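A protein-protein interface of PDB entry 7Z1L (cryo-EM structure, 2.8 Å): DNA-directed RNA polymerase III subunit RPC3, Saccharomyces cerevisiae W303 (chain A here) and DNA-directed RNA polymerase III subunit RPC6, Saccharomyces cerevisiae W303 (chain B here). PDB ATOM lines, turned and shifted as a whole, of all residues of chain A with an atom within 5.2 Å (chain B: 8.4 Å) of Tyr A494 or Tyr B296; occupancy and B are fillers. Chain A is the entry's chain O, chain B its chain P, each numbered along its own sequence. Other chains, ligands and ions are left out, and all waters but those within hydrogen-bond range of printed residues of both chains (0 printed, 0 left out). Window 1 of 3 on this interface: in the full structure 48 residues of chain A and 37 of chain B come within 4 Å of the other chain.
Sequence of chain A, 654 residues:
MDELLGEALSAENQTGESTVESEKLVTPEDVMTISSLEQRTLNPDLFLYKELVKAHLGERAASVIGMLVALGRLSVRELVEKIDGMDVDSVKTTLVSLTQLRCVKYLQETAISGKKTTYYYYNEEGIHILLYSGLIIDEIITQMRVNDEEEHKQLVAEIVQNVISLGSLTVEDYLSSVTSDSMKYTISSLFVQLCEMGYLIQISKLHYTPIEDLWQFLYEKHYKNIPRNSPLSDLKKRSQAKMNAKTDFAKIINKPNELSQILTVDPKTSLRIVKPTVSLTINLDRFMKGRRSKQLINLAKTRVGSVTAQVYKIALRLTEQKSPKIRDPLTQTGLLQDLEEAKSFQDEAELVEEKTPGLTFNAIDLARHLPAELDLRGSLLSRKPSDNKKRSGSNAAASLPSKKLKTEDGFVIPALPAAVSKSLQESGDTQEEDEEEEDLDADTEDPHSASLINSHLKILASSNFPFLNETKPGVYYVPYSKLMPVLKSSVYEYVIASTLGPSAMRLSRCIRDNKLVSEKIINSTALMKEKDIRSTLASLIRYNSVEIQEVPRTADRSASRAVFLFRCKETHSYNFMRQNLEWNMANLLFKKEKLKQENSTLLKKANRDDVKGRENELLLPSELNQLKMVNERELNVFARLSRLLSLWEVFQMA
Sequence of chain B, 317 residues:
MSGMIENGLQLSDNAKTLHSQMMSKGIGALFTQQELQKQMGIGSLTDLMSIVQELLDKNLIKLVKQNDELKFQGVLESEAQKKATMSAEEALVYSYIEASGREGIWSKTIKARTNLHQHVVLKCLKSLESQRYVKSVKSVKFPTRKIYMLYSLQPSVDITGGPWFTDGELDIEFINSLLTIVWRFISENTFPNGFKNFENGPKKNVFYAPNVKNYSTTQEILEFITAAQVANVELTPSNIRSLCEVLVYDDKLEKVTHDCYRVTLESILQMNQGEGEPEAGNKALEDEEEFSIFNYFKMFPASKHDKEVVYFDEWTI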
ATOM      1  N   ARG A 303     -15.780 -13.881 -21.217  1.00  0.00           N
ATOM      2  CA  ARG A 303     -16.483 -12.705 -21.714  1.00  0.00           C
ATOM      3  C   ARG A 303     -17.990 -12.885 -21.740  1.00  0.00           C
ATOM      4  O   ARG A 303     -18.720 -12.018 -21.245  1.00  0.00           O
ATOM      5  CB  ARG A 303     -15.977 -12.341 -23.120  1.00  0.00           C
ATOM      6  CG  ARG A 303     -14.504 -11.983 -23.177  1.00  0.00           C
ATOM      7  CD  ARG A 303     -14.227 -10.666 -22.474  1.00  0.00           C
ATOM      8  NE  ARG A 303     -12.942 -10.678 -21.788  1.00  0.00           N
ATOM      9  CZ  ARG A 303     -12.390  -9.618 -21.215  1.00  0.00           C
ATOM     10  NH1 ARG A 303     -12.981  -8.435 -21.234  1.00  0.00           N
ATOM     11  NH2 ARG A 303     -11.212  -9.748 -20.610  1.00  0.00           N
ATOM     12  N   SER A 489      -3.332 -10.591 -27.675  1.00  0.00           N
ATOM     13  CA  SER A 489      -3.238  -9.438 -26.785  1.00  0.00           C
ATOM     14  C   SER A 489      -3.775  -9.768 -25.399  1.00  0.00           C
ATOM     15  O   SER A 489      -3.168  -9.403 -24.387  1.00  0.00           O
ATOM     16  CB  SER A 489      -3.990  -8.252 -27.387  1.00  0.00           C
ATOM     17  OG  SER A 489      -4.025  -7.163 -26.483  1.00  0.00           O
ATOM     18  N   SER A 490      -4.909 -10.474 -25.334  1.00  0.00           N
ATOM     19  CA  SER A 490      -5.495 -10.816 -24.041  1.00  0.00           C
ATOM     20  C   SER A 490      -4.605 -11.775 -23.260  1.00  0.00           C
ATOM     21  O   SER A 490      -4.393 -11.589 -22.055  1.00  0.00           O
ATOM     22  CB  SER A 490      -6.885 -11.415 -24.239  1.00  0.00           C
ATOM     23  OG  SER A 490      -7.853 -10.398 -24.417  1.00  0.00           O
ATOM     24  N   VAL A 491      -4.065 -12.797 -23.931  1.00  0.00           N
ATOM     25  CA  VAL A 491      -3.200 -13.760 -23.253  1.00  0.00           C
ATOM     26  C   VAL A 491      -1.929 -13.083 -22.756  1.00  0.00           C
ATOM     27  O   VAL A 491      -1.499 -13.300 -21.617  1.00  0.00           O
ATOM     28  CB  VAL A 491      -2.892 -14.947 -24.185  1.00  0.00           C
ATOM     29  CG1 VAL A 491      -1.756 -15.783 -23.633  1.00  0.00           C
ATOM     30  CG2 VAL A 491      -4.130 -15.803 -24.366  1.00  0.00           C
ATOM     31  N   TYR A 492      -1.324 -12.232 -23.589  1.00  0.00           N
ATOM     32  CA  TYR A 492      -0.108 -11.526 -23.195  1.00  0.00           C
ATOM     33  C   TYR A 492      -0.363 -10.575 -22.029  1.00  0.00           C
ATOM     34  O   TYR A 492       0.419 -10.529 -21.065  1.00  0.00           O
ATOM     35  CB  TYR A 492       0.442 -10.784 -24.411  1.00  0.00           C
ATOM     36  CG  TYR A 492       1.519  -9.776 -24.126  1.00  0.00           C
ATOM     37  CD1 TYR A 492       2.830 -10.172 -23.912  1.00  0.00           C
ATOM     38  CD2 TYR A 492       1.230  -8.420 -24.103  1.00  0.00           C
ATOM     39  CE1 TYR A 492       3.816  -9.250 -23.660  1.00  0.00           C
ATOM     40  CE2 TYR A 492       2.208  -7.492 -23.854  1.00  0.00           C
ATOM     41  CZ  TYR A 492       3.500  -7.911 -23.639  1.00  0.00           C
ATOM     42  OH  TYR A 492       4.473  -6.981 -23.382  1.00  0.00           O
ATOM     43  N   GLU A 493      -1.470  -9.828 -22.085  1.00  0.00           N
ATOM     44  CA  GLU A 493      -1.797  -8.895 -21.014  1.00  0.00           C
ATOM     45  C   GLU A 493      -2.078  -9.625 -19.709  1.00  0.00           C
ATOM     46  O   GLU A 493      -1.689  -9.157 -18.635  1.00  0.00           O
ATOM     47  CB  GLU A 493      -2.996  -8.038 -21.414  1.00  0.00           C
ATOM     48  CG  GLU A 493      -2.655  -6.885 -22.339  1.00  0.00           C
ATOM     49  CD  GLU A 493      -3.884  -6.275 -22.982  1.00  0.00           C
ATOM     50  OE1 GLU A 493      -4.982  -6.396 -22.399  1.00  0.00           O
ATOM     51  OE2 GLU A 493      -3.753  -5.678 -24.071  1.00  0.00           O
ATOM     52  N   TYR A 494      -2.743 -10.781 -19.775  1.00  0.00           N
ATOM     53  CA  TYR A 494      -3.041 -11.491 -18.538  1.00  0.00           C
ATOM     54  C   TYR A 494      -1.818 -12.218 -17.994  1.00  0.00           C
ATOM     55  O   TYR A 494      -1.704 -12.393 -16.777  1.00  0.00           O
ATOM     56  CB  TYR A 494      -4.215 -12.443 -18.744  1.00  0.00           C
ATOM     57  CG  TYR A 494      -5.536 -11.746 -18.512  1.00  0.00           C
ATOM     58  CD1 TYR A 494      -5.944 -10.714 -19.345  1.00  0.00           C
ATOM     59  CD2 TYR A 494      -6.354 -12.089 -17.446  1.00  0.00           C
ATOM     60  CE1 TYR A 494      -7.135 -10.059 -19.140  1.00  0.00           C
ATOM     61  CE2 TYR A 494      -7.554 -11.435 -17.230  1.00  0.00           C
ATOM     62  CZ  TYR A 494      -7.937 -10.421 -18.084  1.00  0.00           C
ATOM     63  OH  TYR A 494      -9.124  -9.756 -17.890  1.00  0.00           O
ATOM     64  N   VAL A 495      -0.880 -12.615 -18.860  1.00  0.00           N
ATOM     65  CA  VAL A 495       0.403 -13.117 -18.371  1.00  0.00           C
ATOM     66  C   VAL A 495       1.140 -12.021 -17.612  1.00  0.00           C
ATOM     67  O   VAL A 495       1.679 -12.254 -16.519  1.00  0.00           O
ATOM     68  CB  VAL A 495       1.248 -13.673 -19.534  1.00  0.00           C
ATOM     69  CG1 VAL A 495       2.692 -13.841 -19.110  1.00  0.00           C
ATOM     70  CG2 VAL A 495       0.701 -15.005 -19.994  1.00  0.00           C
ATOM     71  N   ILE A 496       1.156 -10.803 -18.165  1.00  0.00           N
ATOM     72  CA  ILE A 496       1.780  -9.680 -17.466  1.00  0.00           C
ATOM     73  C   ILE A 496       1.064  -9.390 -16.150  1.00  0.00           C
ATOM     74  O   ILE A 496       1.704  -9.142 -15.122  1.00  0.00           O
ATOM     75  CB  ILE A 496       1.827  -8.435 -18.373  1.00  0.00           C
ATOM     76  CG1 ILE A 496       2.897  -8.597 -19.444  1.00  0.00           C
ATOM     77  CG2 ILE A 496       2.085  -7.176 -17.574  1.00  0.00           C
ATOM     78  CD1 ILE A 496       2.970  -7.418 -20.357  1.00  0.00           C
ATOM     79  N   ALA A 497      -0.270  -9.431 -16.157  1.00  0.00           N
ATOM     80  CA  ALA A 497      -1.031  -9.166 -14.939  1.00  0.00           C
ATOM     81  C   ALA A 497      -0.753 -10.210 -13.867  1.00  0.00           C
ATOM     82  O   ALA A 497      -0.663  -9.883 -12.679  1.00  0.00           O
ATOM     83  CB  ALA A 497      -2.524  -9.116 -15.252  1.00  0.00           C
ATOM     84  N   SER A 498      -0.620 -11.473 -14.265  1.00  0.00           N
ATOM     85  CA  SER A 498      -0.374 -12.534 -13.299  1.00  0.00           C
ATOM     86  C   SER A 498       1.055 -12.521 -12.775  1.00  0.00           C
ATOM     87  O   SER A 498       1.284 -12.895 -11.619  1.00  0.00           O
ATOM     88  CB  SER A 498      -0.687 -13.888 -13.928  1.00  0.00           C
ATOM     89  OG  SER A 498       0.213 -14.179 -14.981  1.00  0.00           O
ATOM     90  N   THR A 499       2.024 -12.104 -13.589  1.00  0.00           N
ATOM     91  CA  THR A 499       3.414 -12.122 -13.143  1.00  0.00           C
ATOM     92  C   THR A 499       3.820 -10.820 -12.457  1.00  0.00           C
ATOM     93  O   THR A 499       4.202 -10.824 -11.282  1.00  0.00           O
ATOM     94  CB  THR A 499       4.342 -12.412 -14.327  1.00  0.00           C
ATOM     95  OG1 THR A 499       4.113 -11.447 -15.362  1.00  0.00           O
ATOM     96  CG2 THR A 499       4.084 -13.803 -14.868  1.00  0.00           C
ATOM     97  N   MET A 505      -0.380  -4.501 -15.970  1.00  0.00           N
ATOM     98  CA  MET A 505      -1.378  -4.615 -17.030  1.00  0.00           C
ATOM     99  C   MET A 505      -2.039  -3.273 -17.309  1.00  0.00           C
ATOM    100  O   MET A 505      -2.270  -2.912 -18.470  1.00  0.00           O
ATOM    101  CB  MET A 505      -2.428  -5.663 -16.662  1.00  0.00           C
ATOM    102  CG  MET A 505      -3.518  -5.819 -17.710  1.00  0.00           C
ATOM    103  SD  MET A 505      -4.670  -7.160 -17.371  1.00  0.00           S
ATOM    104  CE  MET A 505      -5.685  -6.407 -16.108  1.00  0.00           C
ATOM    105  N   TYR B 249      -9.030   0.438 -18.441  1.00  0.00           N
ATOM    106  CA  TYR B 249      -7.610   0.105 -18.517  1.00  0.00           C
ATOM    107  C   TYR B 249      -7.272  -1.084 -17.624  1.00  0.00           C
ATOM    108  O   TYR B 249      -6.400  -1.893 -17.960  1.00  0.00           O
ATOM    109  CB  TYR B 249      -6.760   1.319 -18.140  1.00  0.00           C
ATOM    110  CG  TYR B 249      -6.620   2.349 -19.239  1.00  0.00           C
ATOM    111  CD1 TYR B 249      -7.249   2.180 -20.466  1.00  0.00           C
ATOM    112  CD2 TYR B 249      -5.865   3.496 -19.045  1.00  0.00           C
ATOM    113  CE1 TYR B 249      -7.126   3.123 -21.466  1.00  0.00           C
ATOM    114  CE2 TYR B 249      -5.736   4.442 -20.039  1.00  0.00           C
ATOM    115  CZ  TYR B 249      -6.368   4.250 -21.247  1.00  0.00           C
ATOM    116  OH  TYR B 249      -6.241   5.192 -22.241  1.00  0.00           O
ATOM    117  N   ASP B 250      -7.954  -1.210 -16.482  1.00  0.00           N
ATOM    118  CA  ASP B 250      -7.782  -2.366 -15.607  1.00  0.00           C
ATOM    119  C   ASP B 250      -8.469  -3.616 -16.137  1.00  0.00           C
ATOM    120  O   ASP B 250      -8.382  -4.665 -15.490  1.00  0.00           O
ATOM    121  CB  ASP B 250      -8.321  -2.064 -14.206  1.00  0.00           C
ATOM    122  CG  ASP B 250      -7.488  -1.045 -13.465  1.00  0.00           C
ATOM    123  OD1 ASP B 250      -6.271  -0.973 -13.723  1.00  0.00           O
ATOM    124  OD2 ASP B 250      -8.047  -0.315 -12.618  1.00  0.00           O
ATOM    125  N   ASP B 251      -9.153  -3.520 -17.278  1.00  0.00           N
ATOM    126  CA  ASP B 251     -10.006  -4.548 -17.864  1.00  0.00           C
ATOM    127  C   ASP B 251     -11.050  -4.964 -16.826  1.00  0.00           C
ATOM    128  O   ASP B 251     -11.218  -6.152 -16.541  1.00  0.00           O
ATOM    129  CB  ASP B 251      -9.164  -5.730 -18.390  1.00  0.00           C
ATOM    130  CG  ASP B 251      -9.974  -6.829 -19.121  1.00  0.00           C
ATOM    131  OD1 ASP B 251     -11.211  -6.952 -19.014  1.00  0.00           O
ATOM    132  OD2 ASP B 251      -9.315  -7.612 -19.838  1.00  0.00           O
ATOM    133  N   LYS B 252     -11.644  -3.995 -16.129  1.00  0.00           N
ATOM    134  CA  LYS B 252     -12.807  -4.292 -15.303  1.00  0.00           C
ATOM    135  C   LYS B 252     -14.082  -4.204 -16.126  1.00  0.00           C
ATOM    136  O   LYS B 252     -15.004  -5.009 -15.951  1.00  0.00           O
ATOM    137  CB  LYS B 252     -12.865  -3.341 -14.109  1.00  0.00           C
ATOM    138  CG  LYS B 252     -11.614  -3.353 -13.246  1.00  0.00           C
ATOM    139  CD  LYS B 252     -11.560  -4.591 -12.369  1.00  0.00           C
ATOM    140  CE  LYS B 252     -12.199  -4.348 -11.014  1.00  0.00           C
ATOM    141  NZ  LYS B 252     -11.477  -3.306 -10.239  1.00  0.00           N
ATOM    142  N   LEU B 253     -14.147  -3.231 -17.031  1.00  0.00           N
ATOM    143  CA  LEU B 253     -15.287  -3.057 -17.918  1.00  0.00           C
ATOM    144  C   LEU B 253     -14.808  -2.859 -19.349  1.00  0.00           C
ATOM    145  O   LEU B 253     -13.625  -3.049 -19.647  1.00  0.00           O
ATOM    146  CB  LEU B 253     -16.155  -1.888 -17.441  1.00  0.00           C
ATOM    147  CG  LEU B 253     -15.532  -0.506 -17.219  1.00  0.00           C
ATOM    148  CD1 LEU B 253     -15.545   0.360 -18.469  1.00  0.00           C
ATOM    149  CD2 LEU B 253     -16.243   0.193 -16.078  1.00  0.00           C
ATOM    150  N   THR B 264     -17.310  -6.308 -17.710  1.00  0.00           N
ATOM    151  CA  THR B 264     -16.945  -7.607 -18.250  1.00  0.00           C
ATOM    152  C   THR B 264     -17.132  -8.702 -17.204  1.00  0.00           C
ATOM    153  O   THR B 264     -17.163  -8.450 -15.998  1.00  0.00           O
ATOM    154  CB  THR B 264     -15.497  -7.595 -18.737  1.00  0.00           C
ATOM    155  OG1 THR B 264     -14.620  -7.429 -17.616  1.00  0.00           O
ATOM    156  CG2 THR B 264     -15.276  -6.451 -19.711  1.00  0.00           C
ATOM    157  N   LEU B 265     -17.252  -9.940 -17.690  1.00  0.00           N
ATOM    158  CA  LEU B 265     -17.480 -11.071 -16.797  1.00  0.00           C
ATOM    159  C   LEU B 265     -16.211 -11.477 -16.056  1.00  0.00           C
ATOM    160  O   LEU B 265     -16.291 -12.046 -14.959  1.00  0.00           O
ATOM    161  CB  LEU B 265     -18.041 -12.252 -17.593  1.00  0.00           C
ATOM    162  CG  LEU B 265     -18.436 -13.519 -16.833  1.00  0.00           C
ATOM    163  CD1 LEU B 265     -19.423 -13.191 -15.727  1.00  0.00           C
ATOM    164  CD2 LEU B 265     -19.016 -14.554 -17.779  1.00  0.00           C
ATOM    165  N   GLU B 266     -15.038 -11.206 -16.636  1.00  0.00           N
ATOM    166  CA  GLU B 266     -13.784 -11.587 -15.991  1.00  0.00           C
ATOM    167  C   GLU B 266     -13.588 -10.844 -14.676  1.00  0.00           C
ATOM    168  O   GLU B 266     -13.147 -11.432 -13.681  1.00  0.00           O
ATOM    169  CB  GLU B 266     -12.610 -11.331 -16.935  1.00  0.00           C
ATOM    170  CG  GLU B 266     -11.247 -11.551 -16.304  1.00  0.00           C
ATOM    171  CD  GLU B 266     -10.998 -12.996 -15.921  1.00  0.00           C
ATOM    172  OE1 GLU B 266     -11.549 -13.898 -16.586  1.00  0.00           O
ATOM    173  OE2 GLU B 266     -10.251 -13.232 -14.950  1.00  0.00           O
ATOM    174  N   SER B 267     -13.918  -9.551 -14.647  1.00  0.00           N
ATOM    175  CA  SER B 267     -13.839  -8.798 -13.400  1.00  0.00           C
ATOM    176  C   SER B 267     -14.838  -9.311 -12.374  1.00  0.00           C
ATOM    177  O   SER B 267     -14.586  -9.226 -11.166  1.00  0.00           O
ATOM    178  CB  SER B 267     -14.071  -7.314 -13.671  1.00  0.00           C
ATOM    179  OG  SER B 267     -15.445  -7.046 -13.874  1.00  0.00           O
ATOM    180  N   GLN B 270     -13.288 -12.364 -10.933  1.00  0.00           N
ATOM    181  CA  GLN B 270     -12.079 -12.065 -10.171  1.00  0.00           C
ATOM    182  C   GLN B 270     -12.389 -11.815  -8.698  1.00  0.00           C
ATOM    183  O   GLN B 270     -11.518 -11.992  -7.837  1.00  0.00           O
ATOM    184  CB  GLN B 270     -11.361 -10.861 -10.779  1.00  0.00           C
ATOM    185  CG  GLN B 270      -9.893 -10.756 -10.404  1.00  0.00           C
ATOM    186  CD  GLN B 270      -9.112  -9.868 -11.351  1.00  0.00           C
ATOM    187  OE1 GLN B 270      -9.678  -9.259 -12.258  1.00  0.00           O
ATOM    188  NE2 GLN B 270      -7.804  -9.789 -11.144  1.00  0.00           N
ATOM    189  N   PHE B 291      -6.795 -25.668 -16.614  1.00  0.00           N
ATOM    190  CA  PHE B 291      -5.975 -24.476 -16.441  1.00  0.00           C
ATOM    191  C   PHE B 291      -6.175 -23.500 -17.593  1.00  0.00           C
ATOM    192  O   PHE B 291      -6.190 -23.892 -18.764  1.00  0.00           O
ATOM    193  CB  PHE B 291      -4.499 -24.848 -16.333  1.00  0.00           C
ATOM    194  CG  PHE B 291      -3.572 -23.672 -16.471  1.00  0.00           C
ATOM    195  CD1 PHE B 291      -3.458 -22.745 -15.451  1.00  0.00           C
ATOM    196  CD2 PHE B 291      -2.822 -23.492 -17.621  1.00  0.00           C
ATOM    197  CE1 PHE B 291      -2.612 -21.659 -15.573  1.00  0.00           C
ATOM    198  CE2 PHE B 291      -1.974 -22.408 -17.749  1.00  0.00           C
ATOM    199  CZ  PHE B 291      -1.870 -21.492 -16.723  1.00  0.00           C
ATOM    200  N   SER B 292      -6.322 -22.223 -17.253  1.00  0.00           N
ATOM    201  CA  SER B 292      -6.311 -21.138 -18.219  1.00  0.00           C
ATOM    202  C   SER B 292      -5.562 -19.968 -17.606  1.00  0.00           C
ATOM    203  O   SER B 292      -5.470 -19.857 -16.380  1.00  0.00           O
ATOM    204  CB  SER B 292      -7.730 -20.716 -18.618  1.00  0.00           C
ATOM    205  OG  SER B 292      -8.412 -21.775 -19.266  1.00  0.00           O
ATOM    206  N   ILE B 293      -5.008 -19.105 -18.459  1.00  0.00           N
ATOM    207  CA  ILE B 293      -4.266 -17.957 -17.956  1.00  0.00           C
ATOM    208  C   ILE B 293      -5.201 -16.904 -17.375  1.00  0.00           C
ATOM    209  O   ILE B 293      -4.796 -16.129 -16.502  1.00  0.00           O
ATOM    210  CB  ILE B 293      -3.372 -17.378 -19.076  1.00  0.00           C
ATOM    211  CG1 ILE B 293      -2.389 -16.350 -18.513  1.00  0.00           C
ATOM    212  CG2 ILE B 293      -4.208 -16.779 -20.195  1.00  0.00           C
ATOM    213  CD1 ILE B 293      -1.549 -16.873 -17.370  1.00  0.00           C
ATOM    214  N   PHE B 294      -6.460 -16.877 -17.815  1.00  0.00           N
ATOM    215  CA  PHE B 294      -7.359 -15.804 -17.407  1.00  0.00           C
ATOM    216  C   PHE B 294      -7.826 -15.979 -15.968  1.00  0.00           C
ATOM    217  O   PHE B 294      -7.956 -14.995 -15.231  1.00  0.00           O
ATOM    218  CB  PHE B 294      -8.542 -15.735 -18.367  1.00  0.00           C
ATOM    219  CG  PHE B 294      -8.139 -15.537 -19.797  1.00  0.00           C
ATOM    220  CD1 PHE B 294      -7.813 -14.278 -20.268  1.00  0.00           C
ATOM    221  CD2 PHE B 294      -8.069 -16.611 -20.666  1.00  0.00           C
ATOM    222  CE1 PHE B 294      -7.435 -14.092 -21.580  1.00  0.00           C
ATOM    223  CE2 PHE B 294      -7.691 -16.432 -21.979  1.00  0.00           C
ATOM    224  CZ  PHE B 294      -7.373 -15.171 -22.437  1.00  0.00           C
ATOM    225  N   ASN B 295      -8.082 -17.215 -15.545  1.00  0.00           N
ATOM    226  CA  ASN B 295      -8.409 -17.489 -14.146  1.00  0.00           C
ATOM    227  C   ASN B 295      -7.149 -17.882 -13.369  1.00  0.00           C
ATOM    228  O   ASN B 295      -7.046 -18.943 -12.756  1.00  0.00           O
ATOM    229  CB  ASN B 295      -9.508 -18.546 -14.054  1.00  0.00           C
ATOM    230  CG  ASN B 295      -9.155 -19.843 -14.763  1.00  0.00           C
ATOM    231  OD1 ASN B 295      -8.044 -20.022 -15.254  1.00  0.00           O
ATOM    232  ND2 ASN B 295     -10.115 -20.757 -14.820  1.00  0.00           N
ATOM    233  N   TYR B 296      -6.175 -16.967 -13.403  1.00  0.00           N
ATOM    234  CA  TYR B 296      -4.904 -17.193 -12.721  1.00  0.00           C
ATOM    235  C   TYR B 296      -5.034 -17.046 -11.211  1.00  0.00           C
ATOM    236  O   TYR B 296      -4.227 -17.611 -10.465  1.00  0.00           O
ATOM    237  CB  TYR B 296      -3.844 -16.230 -13.260  1.00  0.00           C
ATOM    238  CG  TYR B 296      -4.156 -14.765 -13.035  1.00  0.00           C
ATOM    239  CD1 TYR B 296      -4.935 -14.054 -13.938  1.00  0.00           C
ATOM    240  CD2 TYR B 296      -3.664 -14.089 -11.926  1.00  0.00           C
ATOM    241  CE1 TYR B 296      -5.221 -12.720 -13.739  1.00  0.00           C
ATOM    242  CE2 TYR B 296      -3.945 -12.753 -11.720  1.00  0.00           C
ATOM    243  CZ  TYR B 296      -4.724 -12.074 -12.631  1.00  0.00           C
ATOM    244  OH  TYR B 296      -5.008 -10.744 -12.432  1.00  0.00           O
ATOM    245  N   PHE B 297      -6.029 -16.286 -10.745  1.00  0.00           N
ATOM    246  CA  PHE B 297      -6.201 -16.088  -9.309  1.00  0.00           C
ATOM    247  C   PHE B 297      -6.643 -17.366  -8.608  1.00  0.00           C
ATOM    248  O   PHE B 297      -6.412 -17.523  -7.405  1.00  0.00           O
ATOM    249  CB  PHE B 297      -7.201 -14.959  -9.054  1.00  0.00           C
ATOM    250  CG  PHE B 297      -8.373 -14.961  -9.995  1.00  0.00           C
ATOM    251  CD1 PHE B 297      -9.436 -15.825  -9.803  1.00  0.00           C
ATOM    252  CD2 PHE B 297      -8.411 -14.089 -11.070  1.00  0.00           C
ATOM    253  CE1 PHE B 297     -10.512 -15.825 -10.669  1.00  0.00           C
ATOM    254  CE2 PHE B 297      -9.483 -14.084 -11.939  1.00  0.00           C
ATOM    255  CZ  PHE B 297     -10.535 -14.954 -11.738  1.00  0.00           C
ATOM    256  N   LYS B 298      -7.277 -18.287  -9.336  1.00  0.00           N
ATOM    257  CA  LYS B 298      -7.674 -19.560  -8.746  1.00  0.00           C
ATOM    258  C   LYS B 298      -6.490 -20.488  -8.519  1.00  0.00           C
ATOM    259  O   LYS B 298      -6.617 -21.461  -7.769  1.00  0.00           O
ATOM    260  CB  LYS B 298      -8.706 -20.254  -9.633  1.00  0.00           C
ATOM    261  CG  LYS B 298     -10.050 -19.551  -9.701  1.00  0.00           C
ATOM    262  CD  LYS B 298     -11.020 -20.322 -10.579  1.00  0.00           C
ATOM    263  CE  LYS B 298     -12.362 -19.618 -10.673  1.00  0.00           C
ATOM    264  NZ  LYS B 298     -13.312 -20.365 -11.541  1.00  0.00           N
ATOM    265  N   MET B 299      -5.349 -20.216  -9.147  1.00  0.00           N
ATOM    266  CA  MET B 299      -4.184 -21.077  -9.018  1.00  0.00           C
ATOM    267  C   MET B 299      -3.440 -20.784  -7.721  1.00  0.00           C
ATOM    268  O   MET B 299      -3.271 -19.626  -7.332  1.00  0.00           O
ATOM    269  CB  MET B 299      -3.250 -20.889 -10.212  1.00  0.00           C
ATOM    270  CG  MET B 299      -3.847 -21.327 -11.539  1.00  0.00           C
ATOM    271  SD  MET B 299      -3.635 -23.091 -11.847  1.00  0.00           S
ATOM    272  CE  MET B 299      -5.339 -23.628 -11.952  1.00  0.00           C
ATOM    273  N   PHE B 300      -2.994 -21.853  -7.051  1.00  0.00           N
ATOM    274  CA  PHE B 300      -2.267 -21.716  -5.799  1.00  0.00           C
ATOM    275  C   PHE B 300      -0.765 -21.635  -6.052  1.00  0.00           C
ATOM    276  O   PHE B 300      -0.255 -22.237  -7.001  1.00  0.00           O
ATOM    277  CB  PHE B 300      -2.564 -22.899  -4.880  1.00  0.00           C
ATOM    278  CG  PHE B 300      -4.008 -23.017  -4.490  1.00  0.00           C
ATOM    279  CD1 PHE B 300      -4.614 -22.035  -3.724  1.00  0.00           C
ATOM    280  CD2 PHE B 300      -4.759 -24.110  -4.887  1.00  0.00           C
ATOM    281  CE1 PHE B 300      -5.944 -22.142  -3.363  1.00  0.00           C
ATOM    282  CE2 PHE B 300      -6.088 -24.223  -4.529  1.00  0.00           C
ATOM    283  CZ  PHE B 300      -6.681 -23.237  -3.765  1.00  0.00           C
ATOM    284  N   PRO B 301      -0.041 -20.882  -5.221  1.00  0.00           N
ATOM    285  CA  PRO B 301       1.421 -20.854  -5.343  1.00  0.00           C
ATOM    286  C   PRO B 301       2.030 -22.205  -5.005  1.00  0.00           C
ATOM    287  O   PRO B 301       1.483 -22.980  -4.217  1.00  0.00           O
ATOM    288  CB  PRO B 301       1.844 -19.780  -4.334  1.00  0.00           C
ATOM    289  CG  PRO B 301       0.611 -18.971  -4.085  1.00  0.00           C
ATOM    290  CD  PRO B 301      -0.529 -19.929  -4.213  1.00  0.00           C
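The guanidinium group of Arg A303 lies within salt-bridge range of the side-chain carboxylate of Asp B251 (3.0 Å).
OD2 of Asp B251 sits at hydrogen-bond distance from OH of Tyr A494 (2.9 Å).
Of the 13 printed residues of chain A, 7 touch a printed residue of chain B.
Hydrophobic or aromatic side chains of chain A that line the printed part of chain B: Val A491, Tyr A494, Val A495 and Met A505.
Along chain A the printed residues that touch a printed residue of chain B span positions 303 to 505.
Of the 21 printed residues of chain B, 8 touch a printed residue of chain A.
Printed residues of chain B that touch a printed residue of chain A: Asp B250, Asp B251, Thr B264, Leu B265, Glu B266, Ile B293, Phe B294 and Tyr B296.
Hydrophobic or aromatic side chains of chain B that line the printed part of chain A: Leu B265, Ile B293, Phe B294 and Tyr B296.
OG of Ser A498 is in hydrogen-bond range of O of Tyr A494, 3.2 Å away.
O of Val A495 is in hydrogen-bond range of OG1 of Thr A499 (2.8 Å).
NH2 of Arg A303 sits at hydrogen-bond distance from OH of Tyr A494, at 3.4 Å.
The backbone carbonyl oxygen (O) of Val A495 sits at hydrogen-bond distance from the side-chain hydroxyl (OG) of Ser A498, at 2.9 Å.
The side-chain hydroxyl of Ser B267 sits at hydrogen-bond distance from the backbone carbonyl oxygen of Thr B264 (3.1 Å).
The backbone carbonyl oxygen of Lys B252 lies within hydrogen-bond range of the side-chain hydroxyl of Thr B264.
Tyr B296 touches two residues of chain A.
Of the printed residues of chain A, Leu B265 touches Arg A303 (3.7 Å).
Of the printed residues of chain B, Val A491 touches Phe B294.
Pro B301 touches none of the printed residues of chain A.
Ser B267 touches none of the printed residues of chain A.
Arg A303 touches Thr B264 (NH1 to CG2, 3.4 Å).
Arg A303 touches Leu B265 (O to CB, 3.7 Å).
Phe B294 touches Ser A490.
CG2 of Val A491 touches CZ of Phe B294 (3.8 Å).
OH of Tyr A494 touches CG of Glu B266 (3.2 Å).
CG of Tyr A494 touches CD1 of Phe B294, 3.8 Å away.
Tyr A494 touches Tyr B296 (CD2 to CE1, 3.9 Å).
Val A495 touches Ile B293 (CG2 to CG1, 3.7 Å).
Tyr B296 touches Ser A498.
CE of Met A505 touches O of Asp B250, 3.3 Å away.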
